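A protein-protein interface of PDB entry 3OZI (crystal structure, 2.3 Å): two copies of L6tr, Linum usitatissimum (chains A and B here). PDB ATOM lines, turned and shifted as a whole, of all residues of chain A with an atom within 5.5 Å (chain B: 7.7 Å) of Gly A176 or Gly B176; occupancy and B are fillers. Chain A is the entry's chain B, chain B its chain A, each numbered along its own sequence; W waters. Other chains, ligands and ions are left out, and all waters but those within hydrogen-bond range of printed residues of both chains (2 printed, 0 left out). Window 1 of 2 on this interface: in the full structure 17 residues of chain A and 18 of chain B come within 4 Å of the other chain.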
ATOM      1  N   LEU A 127      10.384  12.877   9.741  1.00  0.00           N
ATOM      2  CA  LEU A 127      11.743  13.206   9.292  1.00  0.00           C
ATOM      3  C   LEU A 127      12.747  12.856  10.368  1.00  0.00           C
ATOM      4  O   LEU A 127      13.017  13.683  11.227  1.00  0.00           O
ATOM      5  CB  LEU A 127      11.886  14.701   9.016  1.00  0.00           C
ATOM      6  CG  LEU A 127      11.225  15.319   7.788  1.00  0.00           C
ATOM      7  CD1 LEU A 127      11.516  16.829   7.745  1.00  0.00           C
ATOM      8  CD2 LEU A 127      11.709  14.630   6.537  1.00  0.00           C
ATOM      9  N   PRO A 128      13.307  11.642  10.323  1.00  0.00           N
ATOM     10  CA  PRO A 128      14.199  11.243  11.411  1.00  0.00           C
ATOM     11  C   PRO A 128      15.574  11.912  11.332  1.00  0.00           C
ATOM     12  O   PRO A 128      16.115  12.130  10.250  1.00  0.00           O
ATOM     13  CB  PRO A 128      14.323   9.727  11.220  1.00  0.00           C
ATOM     14  CG  PRO A 128      14.109   9.518   9.737  1.00  0.00           C
ATOM     15  CD  PRO A 128      13.077  10.554   9.351  1.00  0.00           C
ATOM     16  N   PHE A 130      19.243  10.946  12.822  1.00  0.00           N
ATOM     17  CA  PHE A 130      19.998   9.944  13.550  1.00  0.00           C
ATOM     18  C   PHE A 130      21.206  10.635  14.182  1.00  0.00           C
ATOM     19  O   PHE A 130      22.202  10.924  13.521  1.00  0.00           O
ATOM     20  CB  PHE A 130      20.375   8.798  12.617  1.00  0.00           C
ATOM     21  CG  PHE A 130      19.197   8.247  11.860  1.00  0.00           C
ATOM     22  CD1 PHE A 130      18.292   7.393  12.484  1.00  0.00           C
ATOM     23  CD2 PHE A 130      18.969   8.610  10.539  1.00  0.00           C
ATOM     24  CE1 PHE A 130      17.187   6.888  11.795  1.00  0.00           C
ATOM     25  CE2 PHE A 130      17.873   8.115   9.837  1.00  0.00           C
ATOM     26  CZ  PHE A 130      16.975   7.252  10.465  1.00  0.00           C
ATOM     27  N   LEU A 174      13.254   5.288   7.180  1.00  0.00           N
ATOM     28  CA  LEU A 174      12.865   6.471   6.418  1.00  0.00           C
ATOM     29  C   LEU A 174      14.118   7.289   6.087  1.00  0.00           C
ATOM     30  O   LEU A 174      15.114   7.230   6.810  1.00  0.00           O
ATOM     31  CB  LEU A 174      11.846   7.319   7.211  1.00  0.00           C
ATOM     32  CG  LEU A 174      10.527   6.632   7.611  1.00  0.00           C
ATOM     33  CD1 LEU A 174       9.619   7.538   8.452  1.00  0.00           C
ATOM     34  CD2 LEU A 174       9.753   6.128   6.370  1.00  0.00           C
ATOM     35  N   LYS A 175      14.071   8.030   4.981  1.00  0.00           N
ATOM     36  CA  LYS A 175      15.146   8.945   4.622  1.00  0.00           C
ATOM     37  C   LYS A 175      15.233  10.064   5.659  1.00  0.00           C
ATOM     38  O   LYS A 175      14.223  10.494   6.215  1.00  0.00           O
ATOM     39  CB  LYS A 175      14.909   9.526   3.230  1.00  0.00           C
ATOM     40  CG  LYS A 175      13.518  10.114   3.060  1.00  0.00           C
ATOM     41  CD  LYS A 175      13.235  10.492   1.603  1.00  0.00           C
ATOM     42  CE  LYS A 175      11.842  11.084   1.471  1.00  0.00           C
ATOM     43  NZ  LYS A 175      11.536  11.393   0.058  1.00  0.00           N
ATOM     44  N   GLY A 176      16.445  10.526   5.929  1.00  0.00           N
ATOM     45  CA  GLY A 176      16.651  11.496   6.982  1.00  0.00           C
ATOM     46  C   GLY A 176      18.092  11.981   6.971  1.00  0.00           C
ATOM     47  O   GLY A 176      18.775  11.922   5.944  1.00  0.00           O
ATOM     48  N   TRP A 177      18.555  12.479   8.112  1.00  0.00           N
ATOM     49  CA  TRP A 177      19.895  13.035   8.194  1.00  0.00           C
ATOM     50  C   TRP A 177      20.616  12.343   9.327  1.00  0.00           C
ATOM     51  O   TRP A 177      20.111  12.279  10.449  1.00  0.00           O
ATOM     52  CB  TRP A 177      19.866  14.534   8.481  1.00  0.00           C
ATOM     53  CG  TRP A 177      19.396  15.413   7.339  1.00  0.00           C
ATOM     54  CD1 TRP A 177      20.175  16.037   6.407  1.00  0.00           C
ATOM     55  CD2 TRP A 177      18.043  15.799   7.053  1.00  0.00           C
ATOM     56  NE1 TRP A 177      19.387  16.768   5.538  1.00  0.00           N
ATOM     57  CE2 TRP A 177      18.078  16.646   5.920  1.00  0.00           C
ATOM     58  CE3 TRP A 177      16.807  15.509   7.642  1.00  0.00           C
ATOM     59  CZ2 TRP A 177      16.932  17.200   5.369  1.00  0.00           C
ATOM     60  CZ3 TRP A 177      15.664  16.069   7.087  1.00  0.00           C
ATOM     61  CH2 TRP A 177      15.735  16.904   5.962  1.00  0.00           C
ATOM     62  N   HIS A 178      21.791  11.816   9.031  1.00  0.00           N
ATOM     63  CA  HIS A 178      22.662  11.369  10.094  1.00  0.00           C
ATOM     64  C   HIS A 178      23.483  12.552  10.589  1.00  0.00           C
ATOM     65  O   HIS A 178      23.894  13.413   9.802  1.00  0.00           O
ATOM     66  CB  HIS A 178      23.585  10.251   9.621  1.00  0.00           C
ATOM     67  CG  HIS A 178      24.470   9.716  10.700  1.00  0.00           C
ATOM     68  ND1 HIS A 178      25.781  10.121  10.862  1.00  0.00           N
ATOM     69  CD2 HIS A 178      24.223   8.824  11.689  1.00  0.00           C
ATOM     70  CE1 HIS A 178      26.300   9.495  11.903  1.00  0.00           C
ATOM     71  NE2 HIS A 178      25.378   8.701  12.419  1.00  0.00           N
ATOM     72  N   ILE B 126      16.415  14.680  -5.443  1.00  0.00           N
ATOM     73  CA  ILE B 126      17.622  13.879  -5.341  1.00  0.00           C
ATOM     74  C   ILE B 126      17.586  13.074  -4.041  1.00  0.00           C
ATOM     75  O   ILE B 126      17.352  13.638  -2.960  1.00  0.00           O
ATOM     76  CB  ILE B 126      18.852  14.779  -5.358  1.00  0.00           C
ATOM     77  CG1 ILE B 126      18.839  15.631  -6.626  1.00  0.00           C
ATOM     78  CG2 ILE B 126      20.126  13.967  -5.277  1.00  0.00           C
ATOM     79  CD1 ILE B 126      19.955  16.680  -6.649  1.00  0.00           C
ATOM     80  N   LEU B 127      17.817  11.762  -4.156  1.00  0.00           N
ATOM     81  CA  LEU B 127      17.713  10.835  -3.031  1.00  0.00           C
ATOM     82  C   LEU B 127      19.041  10.109  -2.810  1.00  0.00           C
ATOM     83  O   LEU B 127      19.276   9.046  -3.391  1.00  0.00           O
ATOM     84  CB  LEU B 127      16.611   9.787  -3.285  1.00  0.00           C
ATOM     85  CG  LEU B 127      15.143  10.216  -3.410  1.00  0.00           C
ATOM     86  CD1 LEU B 127      14.255   9.039  -3.798  1.00  0.00           C
ATOM     87  CD2 LEU B 127      14.666  10.867  -2.125  1.00  0.00           C
ATOM     88  N   PRO B 128      19.911  10.676  -1.969  1.00  0.00           N
ATOM     89  CA  PRO B 128      21.243  10.089  -1.778  1.00  0.00           C
ATOM     90  C   PRO B 128      21.239   8.823  -0.941  1.00  0.00           C
ATOM     91  O   PRO B 128      20.576   8.753   0.088  1.00  0.00           O
ATOM     92  CB  PRO B 128      22.012  11.195  -1.049  1.00  0.00           C
ATOM     93  CG  PRO B 128      20.945  11.947  -0.289  1.00  0.00           C
ATOM     94  CD  PRO B 128      19.725  11.916  -1.194  1.00  0.00           C
ATOM     95  N   ILE B 129      21.991   7.828  -1.401  1.00  0.00           N
ATOM     96  CA  ILE B 129      22.311   6.672  -0.588  1.00  0.00           C
ATOM     97  C   ILE B 129      23.780   6.768  -0.147  1.00  0.00           C
ATOM     98  O   ILE B 129      24.681   6.846  -0.969  1.00  0.00           O
ATOM     99  CB  ILE B 129      22.078   5.358  -1.361  1.00  0.00           C
ATOM    100  CG1 ILE B 129      20.725   5.397  -2.091  1.00  0.00           C
ATOM    101  CG2 ILE B 129      22.170   4.165  -0.419  1.00  0.00           C
ATOM    102  CD1 ILE B 129      19.499   5.301  -1.168  1.00  0.00           C
ATOM    103  N   PHE B 130      24.005   6.786   1.158  1.00  0.00           N
ATOM    104  CA  PHE B 130      25.351   6.849   1.701  1.00  0.00           C
ATOM    105  C   PHE B 130      25.833   5.424   1.973  1.00  0.00           C
ATOM    106  O   PHE B 130      25.531   4.838   3.017  1.00  0.00           O
ATOM    107  CB  PHE B 130      25.351   7.711   2.961  1.00  0.00           C
ATOM    108  CG  PHE B 130      24.856   9.102   2.714  1.00  0.00           C
ATOM    109  CD1 PHE B 130      25.675  10.039   2.103  1.00  0.00           C
ATOM    110  CD2 PHE B 130      23.552   9.457   3.026  1.00  0.00           C
ATOM    111  CE1 PHE B 130      25.214  11.328   1.833  1.00  0.00           C
ATOM    112  CE2 PHE B 130      23.075  10.745   2.756  1.00  0.00           C
ATOM    113  CZ  PHE B 130      23.903  11.683   2.154  1.00  0.00           C
ATOM    114  N   PRO B 135      28.247  10.226   6.148  1.00  0.00           N
ATOM    115  CA  PRO B 135      27.729  11.415   5.460  1.00  0.00           C
ATOM    116  C   PRO B 135      28.633  12.634   5.647  1.00  0.00           C
ATOM    117  O   PRO B 135      28.798  13.399   4.702  1.00  0.00           O
ATOM    118  CB  PRO B 135      26.371  11.620   6.128  1.00  0.00           C
ATOM    119  CG  PRO B 135      25.932  10.187   6.450  1.00  0.00           C
ATOM    120  CD  PRO B 135      27.197   9.497   6.881  1.00  0.00           C
ATOM    121  N   ARG B 139      29.796  15.211   2.775  1.00  0.00           N
ATOM    122  CA  ARG B 139      29.508  16.624   3.001  1.00  0.00           C
ATOM    123  C   ARG B 139      30.738  17.529   2.945  1.00  0.00           C
ATOM    124  O   ARG B 139      30.649  18.661   2.468  1.00  0.00           O
ATOM    125  CB  ARG B 139      28.815  16.804   4.359  1.00  0.00           C
ATOM    126  CG  ARG B 139      27.352  16.340   4.405  1.00  0.00           C
ATOM    127  CD  ARG B 139      26.913  16.099   5.852  1.00  0.00           C
ATOM    128  NE  ARG B 139      25.563  15.546   5.929  1.00  0.00           N
ATOM    129  CZ  ARG B 139      25.059  14.978   7.019  1.00  0.00           C
ATOM    130  NH1 ARG B 139      25.796  14.890   8.128  1.00  0.00           N
ATOM    131  NH2 ARG B 139      23.823  14.498   7.005  1.00  0.00           N
ATOM    132  N   VAL B 171      24.435  17.558  -2.111  1.00  0.00           N
ATOM    133  CA  VAL B 171      23.771  16.255  -2.031  1.00  0.00           C
ATOM    134  C   VAL B 171      23.975  15.584  -0.674  1.00  0.00           C
ATOM    135  O   VAL B 171      23.060  14.978  -0.139  1.00  0.00           O
ATOM    136  CB  VAL B 171      24.244  15.288  -3.145  1.00  0.00           C
ATOM    137  CG1 VAL B 171      23.669  13.894  -2.912  1.00  0.00           C
ATOM    138  CG2 VAL B 171      23.870  15.819  -4.538  1.00  0.00           C
ATOM    139  N   GLY B 172      25.180  15.675  -0.123  1.00  0.00           N
ATOM    140  CA  GLY B 172      25.446  15.126   1.202  1.00  0.00           C
ATOM    141  C   GLY B 172      24.579  15.699   2.316  1.00  0.00           C
ATOM    142  O   GLY B 172      24.327  15.024   3.324  1.00  0.00           O
ATOM    143  N   ASP B 173      24.126  16.940   2.133  1.00  0.00           N
ATOM    144  CA  ASP B 173      23.235  17.625   3.081  1.00  0.00           C
ATOM    145  C   ASP B 173      21.738  17.339   2.902  1.00  0.00           C
ATOM    146  O   ASP B 173      20.925  17.918   3.620  1.00  0.00           O
ATOM    147  CB  ASP B 173      23.419  19.150   2.987  1.00  0.00           C
ATOM    148  CG  ASP B 173      24.607  19.647   3.788  1.00  0.00           C
ATOM    149  OD1 ASP B 173      25.125  18.864   4.604  1.00  0.00           O
ATOM    150  OD2 ASP B 173      25.008  20.826   3.621  1.00  0.00           O
ATOM    151  N   LEU B 174      21.374  16.487   1.941  1.00  0.00           N
ATOM    152  CA  LEU B 174      19.964  16.149   1.702  1.00  0.00           C
ATOM    153  C   LEU B 174      19.584  14.925   2.514  1.00  0.00           C
ATOM    154  O   LEU B 174      20.435  14.094   2.815  1.00  0.00           O
ATOM    155  CB  LEU B 174      19.722  15.857   0.211  1.00  0.00           C
ATOM    156  CG  LEU B 174      20.047  16.989  -0.773  1.00  0.00           C
ATOM    157  CD1 LEU B 174      19.813  16.528  -2.215  1.00  0.00           C
ATOM    158  CD2 LEU B 174      19.186  18.223  -0.483  1.00  0.00           C
ATOM    159  N   LYS B 175      18.308  14.795   2.853  1.00  0.00           N
ATOM    160  CA  LYS B 175      17.822  13.568   3.494  1.00  0.00           C
ATOM    161  C   LYS B 175      17.981  12.353   2.569  1.00  0.00           C
ATOM    162  O   LYS B 175      17.861  12.444   1.339  1.00  0.00           O
ATOM    163  CB  LYS B 175      16.374  13.730   3.959  1.00  0.00           C
ATOM    164  CG  LYS B 175      15.437  14.094   2.838  1.00  0.00           C
ATOM    165  CD  LYS B 175      14.082  14.512   3.372  1.00  0.00           C
ATOM    166  CE  LYS B 175      13.145  14.900   2.241  1.00  0.00           C
ATOM    167  NZ  LYS B 175      11.780  15.233   2.747  1.00  0.00           N
ATOM    168  N   GLY B 176      18.276  11.212   3.163  1.00  0.00           N
ATOM    169  CA  GLY B 176      18.611  10.038   2.385  1.00  0.00           C
ATOM    170  C   GLY B 176      18.713   8.825   3.280  1.00  0.00           C
ATOM    171  O   GLY B 176      18.219   8.835   4.401  1.00  0.00           O
ATOM    172  N   TRP B 177      19.340   7.768   2.780  1.00  0.00           N
ATOM    173  CA  TRP B 177      19.498   6.559   3.569  1.00  0.00           C
ATOM    174  C   TRP B 177      20.969   6.212   3.678  1.00  0.00           C
ATOM    175  O   TRP B 177      21.706   6.253   2.688  1.00  0.00           O
ATOM    176  CB  TRP B 177      18.778   5.368   2.929  1.00  0.00           C
ATOM    177  CG  TRP B 177      17.277   5.428   2.929  1.00  0.00           C
ATOM    178  CD1 TRP B 177      16.427   4.850   3.832  1.00  0.00           C
ATOM    179  CD2 TRP B 177      16.448   6.073   1.953  1.00  0.00           C
ATOM    180  NE1 TRP B 177      15.122   5.104   3.479  1.00  0.00           N
ATOM    181  CE2 TRP B 177      15.105   5.852   2.331  1.00  0.00           C
ATOM    182  CE3 TRP B 177      16.710   6.812   0.793  1.00  0.00           C
ATOM    183  CZ2 TRP B 177      14.027   6.336   1.588  1.00  0.00           C
ATOM    184  CZ3 TRP B 177      15.628   7.305   0.057  1.00  0.00           C
ATOM    185  CH2 TRP B 177      14.309   7.067   0.466  1.00  0.00           C
ATOM    186  N   HIS B 178      21.383   5.832   4.875  1.00  0.00           N
ATOM    187  CA  HIS B 178      22.712   5.287   5.064  1.00  0.00           C
ATOM    188  C   HIS B 178      22.693   3.764   5.007  1.00  0.00           C
ATOM    189  O   HIS B 178      21.779   3.112   5.505  1.00  0.00           O
ATOM    190  CB  HIS B 178      23.309   5.739   6.392  1.00  0.00           C
ATOM    191  CG  HIS B 178      24.689   5.214   6.626  1.00  0.00           C
ATOM    192  ND1 HIS B 178      24.940   4.095   7.390  1.00  0.00           N
ATOM    193  CD2 HIS B 178      25.890   5.633   6.162  1.00  0.00           C
ATOM    194  CE1 HIS B 178      26.240   3.861   7.407  1.00  0.00           C
ATOM    195  NE2 HIS B 178      26.839   4.781   6.670  1.00  0.00           N
ATOM    196  N   ILE B 179      23.716   3.192   4.392  1.00  0.00           N
ATOM    197  CA  ILE B 179      23.889   1.752   4.455  1.00  0.00           C
ATOM    198  C   ILE B 179      25.201   1.380   5.139  1.00  0.00           C
ATOM    199  O   ILE B 179      26.267   1.863   4.773  1.00  0.00           O
ATOM    200  CB  ILE B 179      23.786   1.135   3.066  1.00  0.00           C
ATOM    201  CG1 ILE B 179      22.352   1.306   2.558  1.00  0.00           C
ATOM    202  CG2 ILE B 179      24.219  -0.328   3.100  1.00  0.00           C
ATOM    203  CD1 ILE B 179      22.065   0.560   1.295  1.00  0.00           C
ATOM    204  N   VAL B 192      13.275   2.133  -0.070  1.00  0.00           N
ATOM    205  CA  VAL B 192      13.550   3.174  -1.051  1.00  0.00           C
ATOM    206  C   VAL B 192      12.628   3.063  -2.272  1.00  0.00           C
ATOM    207  O   VAL B 192      12.086   4.069  -2.739  1.00  0.00           O
ATOM    208  CB  VAL B 192      15.013   3.136  -1.513  1.00  0.00           C
ATOM    209  CG1 VAL B 192      15.259   4.216  -2.555  1.00  0.00           C
ATOM    210  CG2 VAL B 192      15.949   3.303  -0.321  1.00  0.00           C
HETATM  211  O   HOH W   1      20.785   9.531   6.281  1.00  0.00           O
HETATM  212  O   HOH W   2      22.459  11.470   6.434  1.00  0.00           O
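Of the 8 printed residues of chain A, 6 touch a printed residue of chain B.
Printed residues of chain A that touch a printed residue of chain B: Leu A127, Leu A174, Lys A175, Gly A176, Trp A177 and His A178.
Hydrophobic or aromatic side chains of chain A that line the printed part of chain B: Leu A127, Trp A177 and His A178.
Hydrophobic or aromatic side chains of chain B within 4 Å of the printed part of chain A: Leu B127, Pro B135 and Trp B177.
Among the printed residues, 12 pairs touch across the chains.
Among the printed residues, no Asp or Glu carboxylate lies within 4 Å of a Lys or Arg side-chain nitrogen of the other chain.
The backbone carbonyl oxygen of Pro B128 sits at hydrogen-bond distance from the backbone NH of Trp B177 (3.1 Å).
N of Phe B130 lies within hydrogen-bond range of O of Trp B177 (2.8 Å).
NE of Arg B139 sits at hydrogen-bond distance from O of Gly B172 (2.9 Å).
The guanidinium group (NE) of Arg B139 is in salt-bridge range of the side-chain carboxylate (OD1) of Asp B173 (3.6 Å).
O of Pro A128 is in hydrogen-bond range of N of Trp A177, at 3.3 Å.
N of Phe A130 is in hydrogen-bond range of O of Trp A177 (2.9 Å).
Leu A127 touches Lys B175, and with the chains exchanged Lys A175 touches Leu B127.
Leu A174 touches Trp B177, and with the chains exchanged Trp A177 touches Leu B174.
Lys A175 touches Trp B177, and with the chains exchanged Trp A177 touches Lys B175.
Gly B176 touches its own counterpart, Gly A176.
8 positions are printed for both chains.
Of the 12 pairs that touch across the chains among the printed residues, 9 have their exchanged pair printed and touching as well.
Printed residues of chain B within 4 Å of Leu A127: Lys B175 (3.8 Å).
Phe A130 touches none of the printed residues of chain B.
Of chain B, only Lys B175 and Gly B176 come within 4 Å of Gly A176.
Printed residues of chain B within 4 Å of His A178: Pro B135 and Arg B139.
Phe B130 touches none of the printed residues of chain A.
Printed residues of chain A within 4 Å of Asp B173: Trp A177 (2.7 Å).
Of the printed residues of chain A, Gly B176 touches Lys A175 and Gly A176.
The nearest residue of chain B that does not touch Gly A176 is Leu B174 (4.2 Å).
The nearest residue of chain A that does not touch Gly B176 is Leu A174 (4.2 Å).
The guanidinium group (NH1) of Arg B139 is in hydrogen-bond range of the backbone carbonyl oxygen (O) of His A178 (2.9 Å).
The backbone carbonyl oxygen (O) of Asp B173 sits at hydrogen-bond distance from the indole nitrogen (NE1) of Trp A177.
O of Gly B176 lies within hydrogen-bond range of N of Gly A176.
The indole nitrogen (NE1) of Trp B177 sits close to the backbone NH (N) of Lys A175, 3.5 Å away.
Lys B175 touches Leu A127 (NZ to CD2, 3.8 Å).
Trp B177 touches Leu A174.
Leu B127 touches Lys A175.
Lys A175 touches Gly B176 (CA to O, 3.1 Å).
Gly A176 touches Lys B175.
Trp A177 touches Leu B174 (NE1 to C, 3.5 Å).
NE1 of Trp A177 touches N of Lys B175 (3.5 Å).
His A178 touches Pro B135.
Water W2 bridges the backbone NH (N) of His A178 (2.7 Å) and the guanidinium group (NH2) of Arg B139 (3.4 Å).
Water W1 bridges the backbone carbonyl oxygen of Gly A176 and the backbone carbonyl oxygen of Gly B176.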
